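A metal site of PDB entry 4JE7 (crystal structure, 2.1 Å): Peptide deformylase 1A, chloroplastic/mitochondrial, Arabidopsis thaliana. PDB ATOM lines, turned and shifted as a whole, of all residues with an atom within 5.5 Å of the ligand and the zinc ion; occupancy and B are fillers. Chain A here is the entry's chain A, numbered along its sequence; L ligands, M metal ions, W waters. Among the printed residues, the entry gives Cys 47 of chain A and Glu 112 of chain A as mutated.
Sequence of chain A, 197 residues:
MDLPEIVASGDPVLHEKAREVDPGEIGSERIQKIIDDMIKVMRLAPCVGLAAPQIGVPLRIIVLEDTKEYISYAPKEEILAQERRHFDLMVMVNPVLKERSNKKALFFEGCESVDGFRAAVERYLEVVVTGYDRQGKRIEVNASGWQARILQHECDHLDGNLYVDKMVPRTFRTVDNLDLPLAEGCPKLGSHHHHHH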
ATOM      1  N   PRO A  46      29.589 -15.008 -31.510  1.00  0.00           N
ATOM      2  CA  PRO A  46      28.676 -15.948 -32.153  1.00  0.00           C
ATOM      3  C   PRO A  46      27.824 -16.655 -31.072  1.00  0.00           C
ATOM      4  O   PRO A  46      28.269 -16.916 -29.942  1.00  0.00           O
ATOM      5  CB  PRO A  46      29.636 -16.950 -32.844  1.00  0.00           C
ATOM      6  CG  PRO A  46      30.854 -16.902 -32.051  1.00  0.00           C
ATOM      7  CD  PRO A  46      30.965 -15.552 -31.438  1.00  0.00           C
ATOM      8  N   CYS A  47      26.588 -16.984 -31.401  1.00  0.00           N
ATOM      9  CA  CYS A  47      25.845 -17.801 -30.487  1.00  0.00           C
ATOM     10  C   CYS A  47      24.993 -18.836 -31.220  1.00  0.00           C
ATOM     11  O   CYS A  47      24.970 -18.872 -32.443  1.00  0.00           O
ATOM     12  CB  CYS A  47      25.129 -16.975 -29.423  1.00  0.00           C
ATOM     13  SG  CYS A  47      23.811 -16.047 -29.995  1.00  0.00           S
ATOM     14  N   VAL A  48      24.346 -19.722 -30.458  1.00  0.00           N
ATOM     15  CA  VAL A  48      23.615 -20.854 -31.035  1.00  0.00           C
ATOM     16  C   VAL A  48      22.104 -20.678 -31.203  1.00  0.00           C
ATOM     17  O   VAL A  48      21.440 -21.580 -31.675  1.00  0.00           O
ATOM     18  CB  VAL A  48      23.894 -22.193 -30.265  1.00  0.00           C
ATOM     19  CG1 VAL A  48      25.364 -22.637 -30.516  1.00  0.00           C
ATOM     20  CG2 VAL A  48      23.526 -22.063 -28.822  1.00  0.00           C
ATOM     21  N   GLY A  49      21.576 -19.525 -30.831  1.00  0.00           N
ATOM     22  CA  GLY A  49      20.153 -19.272 -31.032  1.00  0.00           C
ATOM     23  C   GLY A  49      19.860 -17.849 -30.665  1.00  0.00           C
ATOM     24  O   GLY A  49      20.680 -17.247 -30.007  1.00  0.00           O
ATOM     25  N   LEU A  50      18.683 -17.349 -31.071  1.00  0.00           N
ATOM     26  CA  LEU A  50      18.230 -15.974 -30.740  1.00  0.00           C
ATOM     27  C   LEU A  50      16.729 -15.871 -30.766  1.00  0.00           C
ATOM     28  O   LEU A  50      16.037 -16.561 -31.539  1.00  0.00           O
ATOM     29  CB  LEU A  50      18.847 -14.939 -31.722  1.00  0.00           C
ATOM     30  CG  LEU A  50      19.363 -13.553 -31.249  1.00  0.00           C
ATOM     31  CD1 LEU A  50      20.719 -13.547 -30.415  1.00  0.00           C
ATOM     32  CD2 LEU A  50      19.548 -12.625 -32.477  1.00  0.00           C
ATOM     33  N   ALA A  51      16.195 -15.021 -29.929  1.00  0.00           N
ATOM     34  CA  ALA A  51      14.786 -14.693 -30.029  1.00  0.00           C
ATOM     35  C   ALA A  51      14.528 -13.228 -30.445  1.00  0.00           C
ATOM     36  O   ALA A  51      15.334 -12.298 -30.129  1.00  0.00           O
ATOM     37  CB  ALA A  51      14.084 -15.031 -28.743  1.00  0.00           C
ATOM     38  N   GLN A  54      15.194 -10.115 -28.305  1.00  0.00           N
ATOM     39  CA  GLN A  54      16.662  -9.837 -28.213  1.00  0.00           C
ATOM     40  C   GLN A  54      17.237  -8.819 -29.187  1.00  0.00           C
ATOM     41  O   GLN A  54      18.287  -8.271 -28.952  1.00  0.00           O
ATOM     42  CB  GLN A  54      17.465 -11.129 -28.280  1.00  0.00           C
ATOM     43  CG  GLN A  54      17.358 -11.940 -27.002  1.00  0.00           C
ATOM     44  CD  GLN A  54      18.121 -13.226 -27.080  1.00  0.00           C
ATOM     45  OE1 GLN A  54      17.726 -14.164 -27.783  1.00  0.00           O
ATOM     46  NE2 GLN A  54      19.260 -13.267 -26.379  1.00  0.00           N
ATOM     47  N   ASP A  66      23.828 -24.710 -34.583  1.00  0.00           N
ATOM     48  CA  ASP A  66      25.008 -25.223 -33.889  1.00  0.00           C
ATOM     49  C   ASP A  66      25.834 -25.990 -34.886  1.00  0.00           C
ATOM     50  O   ASP A  66      25.508 -27.118 -35.260  1.00  0.00           O
ATOM     51  CB  ASP A  66      24.679 -26.181 -32.750  1.00  0.00           C
ATOM     52  CG  ASP A  66      25.724 -26.201 -31.651  1.00  0.00           C
ATOM     53  OD1 ASP A  66      25.477 -26.867 -30.624  1.00  0.00           O
ATOM     54  OD2 ASP A  66      26.790 -25.567 -31.793  1.00  0.00           O
ATOM     55  N   TYR A  70      31.612 -24.615 -34.246  1.00  0.00           N
ATOM     56  CA  TYR A  70      31.461 -24.185 -32.863  1.00  0.00           C
ATOM     57  C   TYR A  70      31.831 -25.356 -31.921  1.00  0.00           C
ATOM     58  O   TYR A  70      32.479 -25.179 -30.882  1.00  0.00           O
ATOM     59  CB  TYR A  70      29.986 -23.793 -32.537  1.00  0.00           C
ATOM     60  CG  TYR A  70      29.345 -22.585 -33.247  1.00  0.00           C
ATOM     61  CD1 TYR A  70      30.116 -21.642 -33.938  1.00  0.00           C
ATOM     62  CD2 TYR A  70      27.955 -22.371 -33.148  1.00  0.00           C
ATOM     63  CE1 TYR A  70      29.529 -20.534 -34.572  1.00  0.00           C
ATOM     64  CE2 TYR A  70      27.356 -21.254 -33.761  1.00  0.00           C
ATOM     65  CZ  TYR A  70      28.153 -20.340 -34.486  1.00  0.00           C
ATOM     66  OH  TYR A  70      27.571 -19.220 -35.131  1.00  0.00           O
ATOM     67  N   ARG A  84      25.399 -33.077 -27.575  1.00  0.00           N
ATOM     68  CA  ARG A  84      25.451 -31.847 -28.346  1.00  0.00           C
ATOM     69  C   ARG A  84      25.823 -32.242 -29.789  1.00  0.00           C
ATOM     70  O   ARG A  84      26.982 -32.627 -30.063  1.00  0.00           O
ATOM     71  CB  ARG A  84      26.532 -30.951 -27.750  1.00  0.00           C
ATOM     72  CG  ARG A  84      26.966 -29.788 -28.636  1.00  0.00           C
ATOM     73  CD  ARG A  84      27.381 -28.555 -27.810  1.00  0.00           C
ATOM     74  NE  ARG A  84      27.465 -27.426 -28.680  1.00  0.00           N
ATOM     75  CZ  ARG A  84      28.232 -26.359 -28.500  1.00  0.00           C
ATOM     76  NH1 ARG A  84      29.006 -26.257 -27.397  1.00  0.00           N
ATOM     77  NH2 ARG A  84      28.211 -25.383 -29.425  1.00  0.00           N
ATOM     78  N   PHE A 108      25.314 -26.026 -17.644  1.00  0.00           N
ATOM     79  CA  PHE A 108      25.473 -24.563 -17.677  1.00  0.00           C
ATOM     80  C   PHE A 108      25.031 -23.913 -18.960  1.00  0.00           C
ATOM     81  O   PHE A 108      25.279 -24.431 -20.031  1.00  0.00           O
ATOM     82  CB  PHE A 108      26.928 -24.171 -17.390  1.00  0.00           C
ATOM     83  CG  PHE A 108      27.271 -24.224 -15.947  1.00  0.00           C
ATOM     84  CD1 PHE A 108      27.845 -25.369 -15.396  1.00  0.00           C
ATOM     85  CD2 PHE A 108      27.001 -23.168 -15.121  1.00  0.00           C
ATOM     86  CE1 PHE A 108      28.174 -25.446 -14.055  1.00  0.00           C
ATOM     87  CE2 PHE A 108      27.288 -23.247 -13.733  1.00  0.00           C
ATOM     88  CZ  PHE A 108      27.898 -24.411 -13.219  1.00  0.00           C
ATOM     89  N   GLU A 109      24.392 -22.745 -18.802  1.00  0.00           N
ATOM     90  CA  GLU A 109      23.925 -21.873 -19.917  1.00  0.00           C
ATOM     91  C   GLU A 109      24.404 -20.446 -19.753  1.00  0.00           C
ATOM     92  O   GLU A 109      24.511 -19.950 -18.666  1.00  0.00           O
ATOM     93  CB  GLU A 109      22.378 -21.810 -19.983  1.00  0.00           C
ATOM     94  CG  GLU A 109      21.647 -23.104 -20.232  1.00  0.00           C
ATOM     95  CD  GLU A 109      20.128 -22.902 -20.496  1.00  0.00           C
ATOM     96  OE1 GLU A 109      19.659 -21.763 -20.745  1.00  0.00           O
ATOM     97  OE2 GLU A 109      19.434 -23.940 -20.512  1.00  0.00           O
ATOM     98  N   GLY A 110      24.652 -19.768 -20.860  1.00  0.00           N
ATOM     99  CA  GLY A 110      24.655 -18.316 -20.842  1.00  0.00           C
ATOM    100  C   GLY A 110      23.628 -17.717 -21.814  1.00  0.00           C
ATOM    101  O   GLY A 110      23.143 -18.409 -22.729  1.00  0.00           O
ATOM    102  N   CYS A 111      23.334 -16.433 -21.605  1.00  0.00           N
ATOM    103  CA  CYS A 111      22.399 -15.695 -22.424  1.00  0.00           C
ATOM    104  C   CYS A 111      23.094 -14.441 -22.959  1.00  0.00           C
ATOM    105  O   CYS A 111      23.792 -13.767 -22.216  1.00  0.00           O
ATOM    106  CB  CYS A 111      21.151 -15.359 -21.620  1.00  0.00           C
ATOM    107  SG  CYS A 111      19.781 -14.546 -22.538  1.00  0.00           S
ATOM    108  N   GLU A 112      22.937 -14.168 -24.250  1.00  0.00           N
ATOM    109  CA  GLU A 112      23.432 -12.918 -24.813  1.00  0.00           C
ATOM    110  C   GLU A 112      22.875 -11.665 -24.133  1.00  0.00           C
ATOM    111  O   GLU A 112      23.442 -10.576 -24.221  1.00  0.00           O
ATOM    112  CB  GLU A 112      23.141 -12.853 -26.307  1.00  0.00           C
ATOM    113  CG  GLU A 112      24.183 -13.666 -27.167  1.00  0.00           C
ATOM    114  CD  GLU A 112      25.669 -13.368 -26.883  1.00  0.00           C
ATOM    115  OE1 GLU A 112      26.428 -14.303 -26.520  1.00  0.00           O
ATOM    116  OE2 GLU A 112      26.086 -12.199 -27.055  1.00  0.00           O
ATOM    117  N   SER A 113      21.745 -11.811 -23.464  1.00  0.00           N
ATOM    118  CA  SER A 113      21.102 -10.690 -22.787  1.00  0.00           C
ATOM    119  C   SER A 113      21.606 -10.456 -21.338  1.00  0.00           C
ATOM    120  O   SER A 113      21.311  -9.418 -20.714  1.00  0.00           O
ATOM    121  CB  SER A 113      19.600 -10.874 -22.863  1.00  0.00           C
ATOM    122  OG  SER A 113      19.216 -10.799 -24.220  1.00  0.00           O
ATOM    123  N   ARG A 118      27.037 -17.262 -16.118  1.00  0.00           N
ATOM    124  CA  ARG A 118      26.493 -18.550 -16.484  1.00  0.00           C
ATOM    125  C   ARG A 118      25.726 -19.135 -15.261  1.00  0.00           C
ATOM    126  O   ARG A 118      25.982 -18.786 -14.127  1.00  0.00           O
ATOM    127  CB  ARG A 118      27.638 -19.503 -16.895  1.00  0.00           C
ATOM    128  CG  ARG A 118      28.653 -18.996 -17.983  1.00  0.00           C
ATOM    129  CD  ARG A 118      27.994 -19.107 -19.387  1.00  0.00           C
ATOM    130  NE  ARG A 118      28.961 -18.860 -20.468  1.00  0.00           N
ATOM    131  CZ  ARG A 118      29.226 -17.645 -20.966  1.00  0.00           C
ATOM    132  NH1 ARG A 118      28.566 -16.558 -20.521  1.00  0.00           N
ATOM    133  NH2 ARG A 118      30.178 -17.499 -21.908  1.00  0.00           N
ATOM    134  N   TRP A 146      21.153 -31.214 -26.681  1.00  0.00           N
ATOM    135  CA  TRP A 146      21.512 -29.814 -26.584  1.00  0.00           C
ATOM    136  C   TRP A 146      20.589 -29.020 -27.445  1.00  0.00           C
ATOM    137  O   TRP A 146      20.180 -27.943 -27.063  1.00  0.00           O
ATOM    138  CB  TRP A 146      22.922 -29.555 -27.072  1.00  0.00           C
ATOM    139  CG  TRP A 146      23.532 -28.313 -26.449  1.00  0.00           C
ATOM    140  CD1 TRP A 146      23.988 -27.220 -27.093  1.00  0.00           C
ATOM    141  CD2 TRP A 146      23.796 -28.095 -25.055  1.00  0.00           C
ATOM    142  NE1 TRP A 146      24.492 -26.293 -26.197  1.00  0.00           N
ATOM    143  CE2 TRP A 146      24.384 -26.806 -24.936  1.00  0.00           C
ATOM    144  CE3 TRP A 146      23.592 -28.869 -23.888  1.00  0.00           C
ATOM    145  CZ2 TRP A 146      24.781 -26.228 -23.668  1.00  0.00           C
ATOM    146  CZ3 TRP A 146      23.985 -28.292 -22.607  1.00  0.00           C
ATOM    147  CH2 TRP A 146      24.563 -26.986 -22.525  1.00  0.00           C
ATOM    148  N   ARG A 149      17.605 -28.218 -25.729  1.00  0.00           N
ATOM    149  CA  ARG A 149      17.940 -27.206 -24.730  1.00  0.00           C
ATOM    150  C   ARG A 149      17.882 -25.835 -25.338  1.00  0.00           C
ATOM    151  O   ARG A 149      17.254 -24.986 -24.764  1.00  0.00           O
ATOM    152  CB  ARG A 149      19.308 -27.490 -24.142  1.00  0.00           C
ATOM    153  CG  ARG A 149      19.898 -26.522 -23.180  1.00  0.00           C
ATOM    154  CD  ARG A 149      20.910 -27.405 -22.400  1.00  0.00           C
ATOM    155  NE  ARG A 149      20.875 -26.830 -21.122  1.00  0.00           N
ATOM    156  CZ  ARG A 149      20.606 -27.352 -19.958  1.00  0.00           C
ATOM    157  NH1 ARG A 149      20.492 -28.651 -19.693  1.00  0.00           N
ATOM    158  NH2 ARG A 149      20.543 -26.447 -19.026  1.00  0.00           N
ATOM    159  N   ILE A 150      18.540 -25.617 -26.473  1.00  0.00           N
ATOM    160  CA  ILE A 150      18.500 -24.304 -27.186  1.00  0.00           C
ATOM    161  C   ILE A 150      17.070 -23.911 -27.506  1.00  0.00           C
ATOM    162  O   ILE A 150      16.667 -22.783 -27.256  1.00  0.00           O
ATOM    163  CB  ILE A 150      19.358 -24.346 -28.502  1.00  0.00           C
ATOM    164  CG1 ILE A 150      20.799 -24.836 -28.220  1.00  0.00           C
ATOM    165  CG2 ILE A 150      19.360 -22.986 -29.286  1.00  0.00           C
ATOM    166  CD1 ILE A 150      21.574 -25.114 -29.528  1.00  0.00           C
ATOM    167  N   HIS A 153      15.414 -22.600 -24.223  1.00  0.00           N
ATOM    168  CA  HIS A 153      15.916 -21.275 -23.873  1.00  0.00           C
ATOM    169  C   HIS A 153      15.303 -20.164 -24.771  1.00  0.00           C
ATOM    170  O   HIS A 153      14.887 -19.092 -24.281  1.00  0.00           O
ATOM    171  CB  HIS A 153      17.429 -21.308 -24.049  1.00  0.00           C
ATOM    172  CG  HIS A 153      18.123 -20.004 -23.765  1.00  0.00           C
ATOM    173  ND1 HIS A 153      18.914 -19.824 -22.655  1.00  0.00           N
ATOM    174  CD2 HIS A 153      18.133 -18.835 -24.444  1.00  0.00           C
ATOM    175  CE1 HIS A 153      19.385 -18.585 -22.656  1.00  0.00           C
ATOM    176  NE2 HIS A 153      18.952 -17.975 -23.741  1.00  0.00           N
ATOM    177  N   GLU A 154      15.267 -20.399 -26.089  1.00  0.00           N
ATOM    178  CA  GLU A 154      14.712 -19.440 -27.041  1.00  0.00           C
ATOM    179  C   GLU A 154      13.215 -19.242 -26.885  1.00  0.00           C
ATOM    180  O   GLU A 154      12.767 -18.094 -26.875  1.00  0.00           O
ATOM    181  CB  GLU A 154      15.010 -19.817 -28.473  1.00  0.00           C
ATOM    182  CG  GLU A 154      16.463 -19.945 -28.788  1.00  0.00           C
ATOM    183  CD  GLU A 154      17.311 -18.762 -28.291  1.00  0.00           C
ATOM    184  OE1 GLU A 154      18.550 -18.985 -28.153  1.00  0.00           O
ATOM    185  OE2 GLU A 154      16.786 -17.629 -28.053  1.00  0.00           O
ATOM    186  N   HIS A 157      12.363 -17.123 -23.968  1.00  0.00           N
ATOM    187  CA  HIS A 157      12.492 -15.686 -24.212  1.00  0.00           C
ATOM    188  C   HIS A 157      11.181 -15.075 -24.716  1.00  0.00           C
ATOM    189  O   HIS A 157      10.907 -13.895 -24.506  1.00  0.00           O
ATOM    190  CB  HIS A 157      13.545 -15.427 -25.304  1.00  0.00           C
ATOM    191  CG  HIS A 157      14.941 -15.225 -24.790  1.00  0.00           C
ATOM    192  ND1 HIS A 157      15.296 -14.180 -23.960  1.00  0.00           N
ATOM    193  CD2 HIS A 157      16.075 -15.908 -25.032  1.00  0.00           C
ATOM    194  CE1 HIS A 157      16.581 -14.231 -23.707  1.00  0.00           C
ATOM    195  NE2 HIS A 157      17.091 -15.259 -24.358  1.00  0.00           N
HETATM  196  C1  LIG L   1      22.048 -17.184 -26.863  1.00  0.00           C
HETATM  197  C2  LIG L   1      20.764 -16.560 -26.257  1.00  0.00           C
HETATM  198  O1  LIG L   1      20.775 -15.794 -25.268  1.00  0.00           O
HETATM  199  N1  LIG L   1      19.653 -16.939 -26.889  1.00  0.00           N
HETATM  200  O2  LIG L   1      18.415 -16.485 -26.474  1.00  0.00           O
HETATM  201  C3  LIG L   1      22.532 -18.477 -26.141  1.00  0.00           C
HETATM  202  C4  LIG L   1      24.002 -18.750 -26.520  1.00  0.00           C
HETATM  203  O3  LIG L   1      24.328 -18.977 -27.690  1.00  0.00           O
HETATM  204  C5  LIG L   1      21.640 -19.710 -26.472  1.00  0.00           C
HETATM  205  C6  LIG L   1      22.011 -20.909 -25.548  1.00  0.00           C
HETATM  206  C7  LIG L   1      20.960 -21.999 -25.560  1.00  0.00           C
HETATM  207  C8  LIG L   1      21.104 -22.963 -24.340  1.00  0.00           C
HETATM  208  C9  LIG L   1      22.508 -23.566 -24.296  1.00  0.00           C
HETATM  209  N2  LIG L   1      24.918 -18.697 -25.531  1.00  0.00           N
HETATM  210  C10 LIG L   1      26.339 -18.886 -25.818  1.00  0.00           C
HETATM  211  C11 LIG L   1      27.201 -18.524 -24.615  1.00  0.00           C
HETATM  212  C12 LIG L   1      26.593 -17.475 -23.693  1.00  0.00           C
HETATM  213  C13 LIG L   1      27.638 -19.739 -23.837  1.00  0.00           C
HETATM  214  C14 LIG L   1      26.621 -20.338 -26.325  1.00  0.00           C
HETATM  215  O4  LIG L   1      25.961 -21.250 -25.784  1.00  0.00           O
HETATM  216  N3  LIG L   1      27.583 -20.519 -27.332  1.00  0.00           N
HETATM  217  C15 LIG L   1      27.986 -21.814 -27.956  1.00  0.00           C
HETATM  218  C16 LIG L   1      28.373 -19.426 -27.955  1.00  0.00           C
HETATM  219  C17 LIG L   1      29.070 -19.978 -29.207  1.00  0.00           C
HETATM  220  C18 LIG L   1      28.874 -21.483 -29.197  1.00  0.00           C
HETATM  221  C19 LIG L   1      28.812 -22.683 -26.998  1.00  0.00           C
HETATM  222  O5  LIG L   1      29.998 -21.948 -26.554  1.00  0.00           O
HETATM  223 ZN    ZN M   1      19.067 -15.961 -24.298  1.00  0.00          ZN
HETATM  224  O   HOH W   1      26.273 -23.848 -26.204  1.00  0.00           O
HETATM  225  O   HOH W   2      32.023 -22.389 -29.134  1.00  0.00           O
HETATM  226  O   HOH W   3      25.214 -21.408 -23.159  1.00  0.00           O
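A nitrogen (N1) of the ligand sits at hydrogen-bond distance from the side-chain carboxylate (OE1) of Glu 154, 2.6 Å away. A nitrogen (N1) of the ligand lies within hydrogen-bond range of the side-chain amide oxygen (OE1) of Gln 54, 3.5 Å away. An oxygen (O3) of the ligand lies close to the side-chain sulfur (SG) of Cys 47, at 3.8 Å. O3 of the ligand lies within hydrogen-bond range of N of Val 48, 2.9 Å away. The backbone NH (N) of Glu 112 sits close to an oxygen (O1) of the ligand (2.9 Å). A nitrogen (N1) of the ligand lies within hydrogen-bond range of the backbone carbonyl oxygen (O) of Gly 49, 3.3 Å away. N2 of the ligand sits at hydrogen-bond distance from O of Gly 110, at 3.3 Å.
ND1 of His 153 is in hydrogen-bond range of OE1 of Glu 109 (2.8 Å). The side-chain sulfur (SG) of Cys 111 lies close to the backbone NH (N) of Ser 113, 3.5 Å away. The side-chain carboxylate (OE1) of Glu 154 lies within hydrogen-bond range of the backbone NH (N) of Leu 50 (3.3 Å). OE2 of Glu 154 lies within hydrogen-bond range of N of Ala 51 (3.3 Å). The side-chain amide nitrogen (NE2) of Gln 54 sits at hydrogen-bond distance from the side-chain hydroxyl (OG) of Ser 113 (3.3 Å). SG of Cys 47 is in hydrogen-bond range of O of Gly 49, 3.4 Å away. The guanidinium group (NH2) of Arg 84 is in salt-bridge range of the side-chain carboxylate (OD2) of Asp 66. The guanidinium group of Arg 149 lies within salt-bridge range of the side-chain carboxylate of Glu 109, 3.1 Å away.
O of Pro 46 touches C16 of the ligand (3.2 Å). Arg 84 touches the ligand. Glu 109 touches the ligand. Arg 118 touches the ligand (NE to C13, 3.7 Å). Trp 146 touches the ligand. CG of Arg 149 touches C8 of the ligand, 3.9 Å away. Ile 150 touches the ligand (CA to C7, 3.7 Å). Hydrophobic or aromatic side chains within 4 Å of the ligand: Val 48, Trp 146, Ile 150, His 153 and His 157. Of the 23 residues printed, 17 come within 4 Å of the ligand. The nearest printed residue that does not touch the ligand is Tyr 70 (4.2 Å).
Gln 54 touches the zinc ion (NE2 to ZN, 3.4 Å).
O1 of the ligand is bound to the zinc ion (2.0 Å). A ring nitrogen (NE2) of His 153 binds the zinc ion (2.1 Å). The zinc ion is bound by NE2 of His 157 (2.1 Å). O2 of the ligand binds the zinc ion, at 2.3 Å. The zinc ion is bound by SG of Cys 111 (2.4 Å). The zinc ion has five donor atoms within binding distance.
Water W1 bridges an oxygen (O4) of the ligand (2.7 Å) and the indole nitrogen (NE1) of Trp 146 (3.0 Å). Water W3 lies within hydrogen-bond range of an oxygen (O4) of the ligand and the backbone NH (N) of Gly 110. Water W2 lies within hydrogen-bond range of an oxygen (O5) of the ligand (3.3 Å) and the backbone carbonyl oxygen of Tyr 70 (3.3 Å).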
